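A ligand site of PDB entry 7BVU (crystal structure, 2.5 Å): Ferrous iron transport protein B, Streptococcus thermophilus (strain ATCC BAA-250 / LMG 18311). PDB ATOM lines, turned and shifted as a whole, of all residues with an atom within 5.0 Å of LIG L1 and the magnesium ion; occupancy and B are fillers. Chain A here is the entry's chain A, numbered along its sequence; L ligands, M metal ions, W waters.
The side-chain amide nitrogen (ND2) of Asn 119 lies within hydrogen-bond range of a nitrogen (N2) of LIG L1, 3.0 Å away. The backbone NH (N) of Lys 20 lies within hydrogen-bond range of an oxygen (O2) of LIG L1. N of Thr 41 lies within hydrogen-bond range of F1 of LG2 L2. O2 of LIG L1 is in salt-bridge range of NZ of Lys 20, 2.6 Å away. The backbone NH of Asn 17 sits at hydrogen-bond distance from a fluorine (F3) of LG2 L2 (2.9 Å). N of Met 120 sits at hydrogen-bond distance from O11 of LIG L1 (3.1 Å). N4 of LIG L1 is in hydrogen-bond range of OD2 of Asp 122 (2.5 Å). N of Ala 149 sits at hydrogen-bond distance from O11 of LIG L1 (2.8 Å). An oxygen (O5) of LIG L1 lies within hydrogen-bond range of the backbone NH (N) of Gly 35, at 3.5 Å. An oxygen (O6) of LIG L1 is in hydrogen-bond range of the backbone NH of Thr 21. N of Asn 17 lies close to O1 of LIG L1, at 3.1 Å. The backbone NH of Ser 18 is in hydrogen-bond range of an oxygen (O2) of LIG L1. An oxygen (O11) of LIG L1 sits close to the side-chain hydroxyl (OG) of Ser 148 (3.2 Å). A fluorine (F1) of LG2 L2 is in hydrogen-bond range of the backbone NH of Val 40 (2.4 Å). The side-chain amino group (NZ) of Lys 20 sits at hydrogen-bond distance from a fluorine (F2) of LG2 L2. The backbone NH (N) of Gly 19 lies within hydrogen-bond range of an oxygen (O4) of LIG L1, at 2.8 Å. OG of Ser 22 lies within hydrogen-bond range of O6 of LIG L1 (2.5 Å). N of Ser 22 lies within hydrogen-bond range of O6 of LIG L1 (2.7 Å).
AL1 of LG2 L2 is bound by O1 of LIG L1, 2.3 Å away.
The backbone NH (N) of Asn 119 lies close to the side-chain hydroxyl (OG1) of Thr 147 (3.3 Å). N of Met 120 lies within hydrogen-bond range of O of Thr 147 (3.2 Å). The backbone NH (N) of Ala 149 lies within hydrogen-bond range of the side-chain amide oxygen (OD1) of Asn 119, 3.3 Å away. The side-chain hydroxyl (OG) of Ser 18 lies within hydrogen-bond range of the backbone carbonyl oxygen (O) of Asn 15, 2.6 Å away. OD2 of Asp 59 lies close to OG1 of Thr 21 (2.7 Å). OD1 of Asn 17 lies close to O of Gly 35, at 3.2 Å. The side-chain amide nitrogen (ND2) of Asn 119 is in hydrogen-bond range of the backbone carbonyl oxygen (O) of Ser 18. The backbone carbonyl oxygen of Asn 36 lies within hydrogen-bond range of the side-chain amide nitrogen of Asn 17 (3.5 Å).
Val 34 touches LIG L1 (CG1 to C3, 3.7 Å). Asn 36 touches LIG L1. Val 123 touches LIG L1 (CG2 to N4, 3.4 Å). Leu 150 touches LIG L1. 16 residues have an atom within 4 Å of LIG L1: Asn 17, Ser 18, Gly 19, Lys 20, Thr 21, Ser 22, Val 34, Gly 35, Asn 36, Asn 119, Met 120, Asp 122, Val 123, Ser 148, Ala 149 and Leu 150. The nearest printed residue that does not touch LIG L1 is Asn 15 (4.03 Å).
Of the 25 residues printed, 2 come within 4 Å of the magnesium ion. Along chain A the residues within 4 Å of the magnesium ion span positions 21 to 41.
The magnesium ion is bound by a fluorine (F4) of LG2 L2 (2.0 Å), the side-chain hydroxyl (OG1) of Thr 21 (2.0 Å), the side-chain hydroxyl (OG1) of Thr 41 (2.1 Å), an oxygen (O3) of LIG L1 (2.3 Å), water W4 (2.3 Å) and water W1 (2.3 Å).
Water W1 lies within hydrogen-bond range of an oxygen (O5) of LIG L1 (2.8 Å) and the backbone carbonyl oxygen of Arg 33 (2.9 Å). Water W4 lies within hydrogen-bond range of the side-chain carboxylate (OD1) of Asp 59 (2.6 Å) and the backbone carbonyl oxygen (O) of Leu 60 (2.7 Å).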
ATOM      1  N   ASN A  15      19.855 -13.303  -4.833  1.00  0.00           N
ATOM      2  CA  ASN A  15      18.737 -13.293  -3.903  1.00  0.00           C
ATOM      3  C   ASN A  15      18.907 -14.405  -2.866  1.00  0.00           C
ATOM      4  O   ASN A  15      19.616 -15.384  -3.091  1.00  0.00           O
ATOM      5  CB  ASN A  15      17.417 -13.476  -4.655  1.00  0.00           C
ATOM      6  CG  ASN A  15      16.980 -12.219  -5.382  1.00  0.00           C
ATOM      7  OD1 ASN A  15      17.686 -11.213  -5.372  1.00  0.00           O
ATOM      8  ND2 ASN A  15      15.825 -12.279  -6.022  1.00  0.00           N
ATOM      9  N   PRO A  16      18.281 -14.250  -1.700  1.00  0.00           N
ATOM     10  CA  PRO A  16      18.243 -15.354  -0.734  1.00  0.00           C
ATOM     11  C   PRO A  16      17.729 -16.644  -1.361  1.00  0.00           C
ATOM     12  O   PRO A  16      16.850 -16.618  -2.228  1.00  0.00           O
ATOM     13  CB  PRO A  16      17.305 -14.830   0.362  1.00  0.00           C
ATOM     14  CG  PRO A  16      17.464 -13.353   0.310  1.00  0.00           C
ATOM     15  CD  PRO A  16      17.709 -13.015  -1.139  1.00  0.00           C
ATOM     16  N   ASN A  17      18.300 -17.765  -0.924  1.00  0.00           N
ATOM     17  CA  ASN A  17      17.843 -19.105  -1.281  1.00  0.00           C
ATOM     18  C   ASN A  17      17.997 -19.414  -2.764  1.00  0.00           C
ATOM     19  O   ASN A  17      17.312 -20.293  -3.292  1.00  0.00           O
ATOM     20  CB  ASN A  17      16.386 -19.338  -0.847  1.00  0.00           C
ATOM     21  CG  ASN A  17      16.195 -20.657  -0.136  1.00  0.00           C
ATOM     22  OD1 ASN A  17      17.137 -21.230   0.397  1.00  0.00           O
ATOM     23  ND2 ASN A  17      14.961 -21.153  -0.137  1.00  0.00           N
ATOM     24  N   SER A  18      18.873 -18.690  -3.470  1.00  0.00           N
ATOM     25  CA  SER A  18      19.091 -18.934  -4.887  1.00  0.00           C
ATOM     26  C   SER A  18      20.130 -20.016  -5.168  1.00  0.00           C
ATOM     27  O   SER A  18      20.316 -20.385  -6.337  1.00  0.00           O
ATOM     28  CB  SER A  18      19.494 -17.640  -5.601  1.00  0.00           C
ATOM     29  OG  SER A  18      20.536 -16.976  -4.901  1.00  0.00           O
ATOM     30  N   GLY A  19      20.804 -20.525  -4.145  1.00  0.00           N
ATOM     31  CA  GLY A  19      21.820 -21.542  -4.326  1.00  0.00           C
ATOM     32  C   GLY A  19      23.258 -21.071  -4.230  1.00  0.00           C
ATOM     33  O   GLY A  19      24.142 -21.754  -4.760  1.00  0.00           O
ATOM     34  N   LYS A  20      23.512 -19.932  -3.574  1.00  0.00           N
ATOM     35  CA  LYS A  20      24.860 -19.385  -3.533  1.00  0.00           C
ATOM     36  C   LYS A  20      25.821 -20.319  -2.793  1.00  0.00           C
ATOM     37  O   LYS A  20      26.883 -20.672  -3.321  1.00  0.00           O
ATOM     38  CB  LYS A  20      24.847 -18.002  -2.896  1.00  0.00           C
ATOM     39  CG  LYS A  20      24.156 -16.948  -3.741  1.00  0.00           C
ATOM     40  CD  LYS A  20      24.190 -15.580  -3.080  1.00  0.00           C
ATOM     41  CE  LYS A  20      23.592 -15.629  -1.683  1.00  0.00           C
ATOM     42  NZ  LYS A  20      22.130 -15.936  -1.699  1.00  0.00           N
ATOM     43  N   THR A  21      25.467 -20.708  -1.567  1.00  0.00           N
ATOM     44  CA  THR A  21      26.353 -21.561  -0.788  1.00  0.00           C
ATOM     45  C   THR A  21      26.479 -22.951  -1.418  1.00  0.00           C
ATOM     46  O   THR A  21      27.542 -23.572  -1.363  1.00  0.00           O
ATOM     47  CB  THR A  21      25.855 -21.669   0.653  1.00  0.00           C
ATOM     48  OG1 THR A  21      25.666 -20.361   1.194  1.00  0.00           O
ATOM     49  CG2 THR A  21      26.863 -22.414   1.519  1.00  0.00           C
ATOM     50  N   SER A  22      25.390 -23.456  -2.011  1.00  0.00           N
ATOM     51  CA  SER A  22      25.453 -24.709  -2.739  1.00  0.00           C
ATOM     52  C   SER A  22      26.515 -24.651  -3.829  1.00  0.00           C
ATOM     53  O   SER A  22      27.315 -25.590  -3.995  1.00  0.00           O
ATOM     54  CB  SER A  22      24.084 -25.051  -3.331  1.00  0.00           C
ATOM     55  OG  SER A  22      23.087 -25.072  -2.327  1.00  0.00           O
ATOM     56  N   ARG A  33      27.117 -24.179   5.521  1.00  0.00           N
ATOM     57  CA  ARG A  33      25.722 -24.480   5.795  1.00  0.00           C
ATOM     58  C   ARG A  33      24.835 -24.152   4.603  1.00  0.00           C
ATOM     59  O   ARG A  33      24.851 -23.036   4.082  1.00  0.00           O
ATOM     60  CB  ARG A  33      25.252 -23.721   7.039  1.00  0.00           C
ATOM     61  CG  ARG A  33      25.889 -24.205   8.325  1.00  0.00           C
ATOM     62  CD  ARG A  33      25.038 -23.867   9.529  1.00  0.00           C
ATOM     63  NE  ARG A  33      25.404 -24.686  10.692  1.00  0.00           N
ATOM     64  CZ  ARG A  33      24.718 -24.717  11.818  1.00  0.00           C
ATOM     65  NH1 ARG A  33      23.621 -23.984  11.966  1.00  0.00           N
ATOM     66  NH2 ARG A  33      25.126 -25.492  12.829  1.00  0.00           N
ATOM     67  N   VAL A  34      24.057 -25.153   4.171  1.00  0.00           N
ATOM     68  CA  VAL A  34      23.085 -25.023   3.093  1.00  0.00           C
ATOM     69  C   VAL A  34      21.736 -25.448   3.641  1.00  0.00           C
ATOM     70  O   VAL A  34      21.630 -26.495   4.295  1.00  0.00           O
ATOM     71  CB  VAL A  34      23.484 -25.869   1.874  1.00  0.00           C
ATOM     72  CG1 VAL A  34      22.318 -25.992   0.898  1.00  0.00           C
ATOM     73  CG2 VAL A  34      24.699 -25.272   1.177  1.00  0.00           C
ATOM     74  N   GLY A  35      20.705 -24.661   3.371  1.00  0.00           N
ATOM     75  CA  GLY A  35      19.368 -24.972   3.838  1.00  0.00           C
ATOM     76  C   GLY A  35      18.333 -24.548   2.832  1.00  0.00           C
ATOM     77  O   GLY A  35      18.503 -23.575   2.096  1.00  0.00           O
ATOM     78  N   ASN A  36      17.220 -25.290   2.811  1.00  0.00           N
ATOM     79  CA  ASN A  36      16.148 -25.049   1.849  1.00  0.00           C
ATOM     80  C   ASN A  36      15.231 -23.900   2.269  1.00  0.00           C
ATOM     81  O   ASN A  36      14.077 -23.863   1.830  1.00  0.00           O
ATOM     82  CB  ASN A  36      15.338 -26.331   1.628  1.00  0.00           C
ATOM     83  CG  ASN A  36      14.756 -26.884   2.905  1.00  0.00           C
ATOM     84  OD1 ASN A  36      15.236 -26.611   3.995  1.00  0.00           O
ATOM     85  ND2 ASN A  36      13.695 -27.687   2.769  1.00  0.00           N
ATOM     86  N   VAL A  40      20.139 -18.690   5.662  1.00  0.00           N
ATOM     87  CA  VAL A  40      21.127 -19.538   6.305  1.00  0.00           C
ATOM     88  C   VAL A  40      22.437 -18.787   6.482  1.00  0.00           C
ATOM     89  O   VAL A  40      22.923 -18.596   7.606  1.00  0.00           O
ATOM     90  CB  VAL A  40      21.333 -20.841   5.504  1.00  0.00           C
ATOM     91  CG1 VAL A  40      22.430 -21.679   6.118  1.00  0.00           C
ATOM     92  CG2 VAL A  40      20.021 -21.627   5.437  1.00  0.00           C
ATOM     93  N   THR A  41      23.042 -18.363   5.371  1.00  0.00           N
ATOM     94  CA  THR A  41      24.283 -17.601   5.416  1.00  0.00           C
ATOM     95  C   THR A  41      24.001 -16.171   5.881  1.00  0.00           C
ATOM     96  O   THR A  41      23.092 -15.508   5.358  1.00  0.00           O
ATOM     97  CB  THR A  41      24.956 -17.586   4.044  1.00  0.00           C
ATOM     98  OG1 THR A  41      25.109 -18.927   3.575  1.00  0.00           O
ATOM     99  CG2 THR A  41      26.323 -16.926   4.127  1.00  0.00           C
ATOM    100  N   ASP A  59      31.472 -16.505  -0.470  1.00  0.00           N
ATOM    101  CA  ASP A  59      30.067 -16.747  -0.188  1.00  0.00           C
ATOM    102  C   ASP A  59      29.520 -15.601   0.657  1.00  0.00           C
ATOM    103  O   ASP A  59      30.160 -15.188   1.626  1.00  0.00           O
ATOM    104  CB  ASP A  59      29.895 -18.085   0.537  1.00  0.00           C
ATOM    105  CG  ASP A  59      28.447 -18.526   0.604  1.00  0.00           C
ATOM    106  OD1 ASP A  59      27.631 -18.042  -0.207  1.00  0.00           O
ATOM    107  OD2 ASP A  59      28.129 -19.368   1.465  1.00  0.00           O
ATOM    108  N   LEU A  60      28.349 -15.111   0.289  1.00  0.00           N
ATOM    109  CA  LEU A  60      27.776 -13.922   0.920  1.00  0.00           C
ATOM    110  C   LEU A  60      26.307 -14.166   1.202  1.00  0.00           C
ATOM    111  O   LEU A  60      25.675 -15.008   0.561  1.00  0.00           O
ATOM    112  CB  LEU A  60      27.973 -12.690   0.037  1.00  0.00           C
ATOM    113  CG  LEU A  60      29.414 -12.184   0.023  1.00  0.00           C
ATOM    114  CD1 LEU A  60      29.726 -11.393  -1.231  1.00  0.00           C
ATOM    115  CD2 LEU A  60      29.695 -11.349   1.262  1.00  0.00           C
ATOM    116  N   ASN A 119      21.059 -20.403 -11.988  1.00  0.00           N
ATOM    117  CA  ASN A 119      21.054 -21.601 -11.175  1.00  0.00           C
ATOM    118  C   ASN A 119      19.645 -22.190 -11.077  1.00  0.00           C
ATOM    119  O   ASN A 119      18.654 -21.574 -11.482  1.00  0.00           O
ATOM    120  CB  ASN A 119      21.602 -21.293  -9.778  1.00  0.00           C
ATOM    121  CG  ASN A 119      22.044 -22.545  -9.030  1.00  0.00           C
ATOM    122  OD1 ASN A 119      22.741 -23.389  -9.584  1.00  0.00           O
ATOM    123  ND2 ASN A 119      21.643 -22.653  -7.771  1.00  0.00           N
ATOM    124  N   MET A 120      19.578 -23.413 -10.542  1.00  0.00           N
ATOM    125  CA  MET A 120      18.327 -24.169 -10.432  1.00  0.00           C
ATOM    126  C   MET A 120      17.689 -24.413 -11.790  1.00  0.00           C
ATOM    127  O   MET A 120      16.468 -24.430 -11.923  1.00  0.00           O
ATOM    128  CB  MET A 120      17.338 -23.479  -9.480  1.00  0.00           C
ATOM    129  CG  MET A 120      17.836 -23.364  -8.057  1.00  0.00           C
ATOM    130  SD  MET A 120      16.547 -22.904  -6.886  1.00  0.00           S
ATOM    131  CE  MET A 120      17.525 -22.671  -5.403  1.00  0.00           C
ATOM    132  N   ILE A 121      18.524 -24.607 -12.816  1.00  0.00           N
ATOM    133  CA  ILE A 121      18.017 -24.877 -14.153  1.00  0.00           C
ATOM    134  C   ILE A 121      17.329 -26.226 -14.239  1.00  0.00           C
ATOM    135  O   ILE A 121      16.483 -26.440 -15.107  1.00  0.00           O
ATOM    136  CB  ILE A 121      19.158 -24.761 -15.184  1.00  0.00           C
ATOM    137  CG1 ILE A 121      18.599 -24.357 -16.559  1.00  0.00           C
ATOM    138  CG2 ILE A 121      19.950 -26.058 -15.280  1.00  0.00           C
ATOM    139  CD1 ILE A 121      17.909 -23.015 -16.567  1.00  0.00           C
ATOM    140  N   ASP A 122      17.677 -27.159 -13.338  1.00  0.00           N
ATOM    141  CA  ASP A 122      16.963 -28.436 -13.291  1.00  0.00           C
ATOM    142  C   ASP A 122      15.507 -28.253 -12.883  1.00  0.00           C
ATOM    143  O   ASP A 122      14.636 -28.986 -13.346  1.00  0.00           O
ATOM    144  CB  ASP A 122      17.667 -29.393 -12.330  1.00  0.00           C
ATOM    145  CG  ASP A 122      17.896 -28.791 -10.963  1.00  0.00           C
ATOM    146  OD1 ASP A 122      18.631 -27.788 -10.865  1.00  0.00           O
ATOM    147  OD2 ASP A 122      17.328 -29.316  -9.975  1.00  0.00           O
ATOM    148  N   VAL A 123      15.238 -27.281 -12.007  1.00  0.00           N
ATOM    149  CA  VAL A 123      13.857 -26.970 -11.639  1.00  0.00           C
ATOM    150  C   VAL A 123      13.073 -26.516 -12.870  1.00  0.00           C
ATOM    151  O   VAL A 123      11.930 -26.931 -13.086  1.00  0.00           O
ATOM    152  CB  VAL A 123      13.821 -25.910 -10.528  1.00  0.00           C
ATOM    153  CG1 VAL A 123      12.439 -25.865  -9.885  1.00  0.00           C
ATOM    154  CG2 VAL A 123      14.884 -26.197  -9.484  1.00  0.00           C
ATOM    155  N   THR A 147      23.150 -23.102 -14.696  1.00  0.00           N
ATOM    156  CA  THR A 147      23.826 -23.918 -13.701  1.00  0.00           C
ATOM    157  C   THR A 147      22.791 -24.712 -12.911  1.00  0.00           C
ATOM    158  O   THR A 147      21.617 -24.356 -12.841  1.00  0.00           O
ATOM    159  CB  THR A 147      24.664 -23.073 -12.728  1.00  0.00           C
ATOM    160  OG1 THR A 147      23.973 -21.858 -12.425  1.00  0.00           O
ATOM    161  CG2 THR A 147      26.026 -22.746 -13.341  1.00  0.00           C
ATOM    162  N   SER A 148      23.254 -25.815 -12.317  1.00  0.00           N
ATOM    163  CA  SER A 148      22.487 -26.529 -11.309  1.00  0.00           C
ATOM    164  C   SER A 148      23.449 -27.069 -10.272  1.00  0.00           C
ATOM    165  O   SER A 148      24.294 -27.918 -10.599  1.00  0.00           O
ATOM    166  CB  SER A 148      21.657 -27.658 -11.933  1.00  0.00           C
ATOM    167  OG  SER A 148      20.868 -28.302 -10.951  1.00  0.00           O
ATOM    168  N   ALA A 149      23.336 -26.595  -9.041  1.00  0.00           N
ATOM    169  CA  ALA A 149      24.184 -27.093  -7.962  1.00  0.00           C
ATOM    170  C   ALA A 149      23.800 -28.497  -7.537  1.00  0.00           C
ATOM    171  O   ALA A 149      24.646 -29.220  -6.985  1.00  0.00           O
ATOM    172  CB  ALA A 149      24.127 -26.148  -6.757  1.00  0.00           C
ATOM    173  N   LEU A 150      22.560 -28.906  -7.784  1.00  0.00           N
ATOM    174  CA  LEU A 150      22.112 -30.242  -7.396  1.00  0.00           C
ATOM    175  C   LEU A 150      22.604 -31.280  -8.392  1.00  0.00           C
ATOM    176  O   LEU A 150      23.192 -32.304  -7.999  1.00  0.00           O
ATOM    177  CB  LEU A 150      20.578 -30.255  -7.303  1.00  0.00           C
ATOM    178  CG  LEU A 150      19.858 -31.412  -6.594  1.00  0.00           C
ATOM    179  CD1 LEU A 150      18.469 -30.949  -6.162  1.00  0.00           C
ATOM    180  CD2 LEU A 150      19.747 -32.647  -7.473  1.00  0.00           C
HETATM  181  P1  LIG L   1      21.768 -19.605  -0.771  1.00  0.00           P
HETATM  182  O1  LIG L   1      20.802 -19.184   0.310  1.00  0.00           O
HETATM  183  O2  LIG L   1      21.795 -18.546  -1.853  1.00  0.00           O
HETATM  184  O3  LIG L   1      23.151 -19.803  -0.190  1.00  0.00           O
HETATM  185  O4  LIG L   1      21.210 -20.985  -1.372  1.00  0.00           O
HETATM  186  P2  LIG L   1      21.526 -22.407  -0.702  1.00  0.00           P
HETATM  187  O5  LIG L   1      21.338 -22.379   0.796  1.00  0.00           O
HETATM  188  O6  LIG L   1      22.910 -22.875  -1.069  1.00  0.00           O
HETATM  189  O7  LIG L   1      20.403 -23.320  -1.410  1.00  0.00           O
HETATM  190  C1  LIG L   1      19.062 -23.260  -0.937  1.00  0.00           C
HETATM  191  C2  LIG L   1      18.307 -24.523  -1.318  1.00  0.00           C
HETATM  192  O8  LIG L   1      18.203 -24.589  -2.744  1.00  0.00           O
HETATM  193  C3  LIG L   1      19.060 -25.760  -0.856  1.00  0.00           C
HETATM  194  O9  LIG L   1      18.123 -26.671  -0.276  1.00  0.00           O
HETATM  195  C4  LIG L   1      19.644 -26.341  -2.126  1.00  0.00           C
HETATM  196  O10 LIG L   1      19.637 -27.770  -2.069  1.00  0.00           O
HETATM  197  C5  LIG L   1      18.689 -25.842  -3.208  1.00  0.00           C
HETATM  198  N1  LIG L   1      19.403 -25.662  -4.500  1.00  0.00           N
HETATM  199  C6  LIG L   1      20.509 -24.920  -4.688  1.00  0.00           C
HETATM  200  N2  LIG L   1      20.903 -24.961  -5.988  1.00  0.00           N
HETATM  201  C7  LIG L   1      20.027 -25.741  -6.640  1.00  0.00           C
HETATM  202  C8  LIG L   1      19.852 -26.207  -8.028  1.00  0.00           C
HETATM  203  O11 LIG L   1      20.651 -25.860  -8.923  1.00  0.00           O
HETATM  204  N3  LIG L   1      18.815 -27.011  -8.310  1.00  0.00           N
HETATM  205  C9  LIG L   1      17.939 -27.400  -7.364  1.00  0.00           C
HETATM  206  N4  LIG L   1      16.920 -28.222  -7.718  1.00  0.00           N
HETATM  207  N5  LIG L   1      18.037 -27.015  -6.066  1.00  0.00           N
HETATM  208  C10 LIG L   1      19.037 -26.203  -5.655  1.00  0.00           C
HETATM  209 AL1  LG2 L   2      20.902 -17.520   1.903  1.00  0.00          AL
HETATM  210  F1  LG2 L   2      20.646 -18.640   3.269  1.00  0.00           F
HETATM  211  F2  LG2 L   2      21.173 -16.408   0.531  1.00  0.00           F
HETATM  212  F3  LG2 L   2      19.145 -17.206   1.834  1.00  0.00           F
HETATM  213  F4  LG2 L   2      22.652 -17.852   1.961  1.00  0.00           F
HETATM  214 MG    MG M   1      24.085 -19.203   1.792  1.00  0.00          MG
HETATM  215  O   HOH W   1      23.193 -21.210   2.525  1.00  0.00           O
HETATM  216  O   HOH W   2      15.147 -26.225  -2.312  1.00  0.00           O
HETATM  217  O   HOH W   3      18.862 -28.540   1.614  1.00  0.00           O
HETATM  218  O   HOH W   4      25.166 -17.641   0.532  1.00  0.00           O
HETATM  219  O   HOH W   5      15.839 -26.685  -4.585  1.00  0.00           O
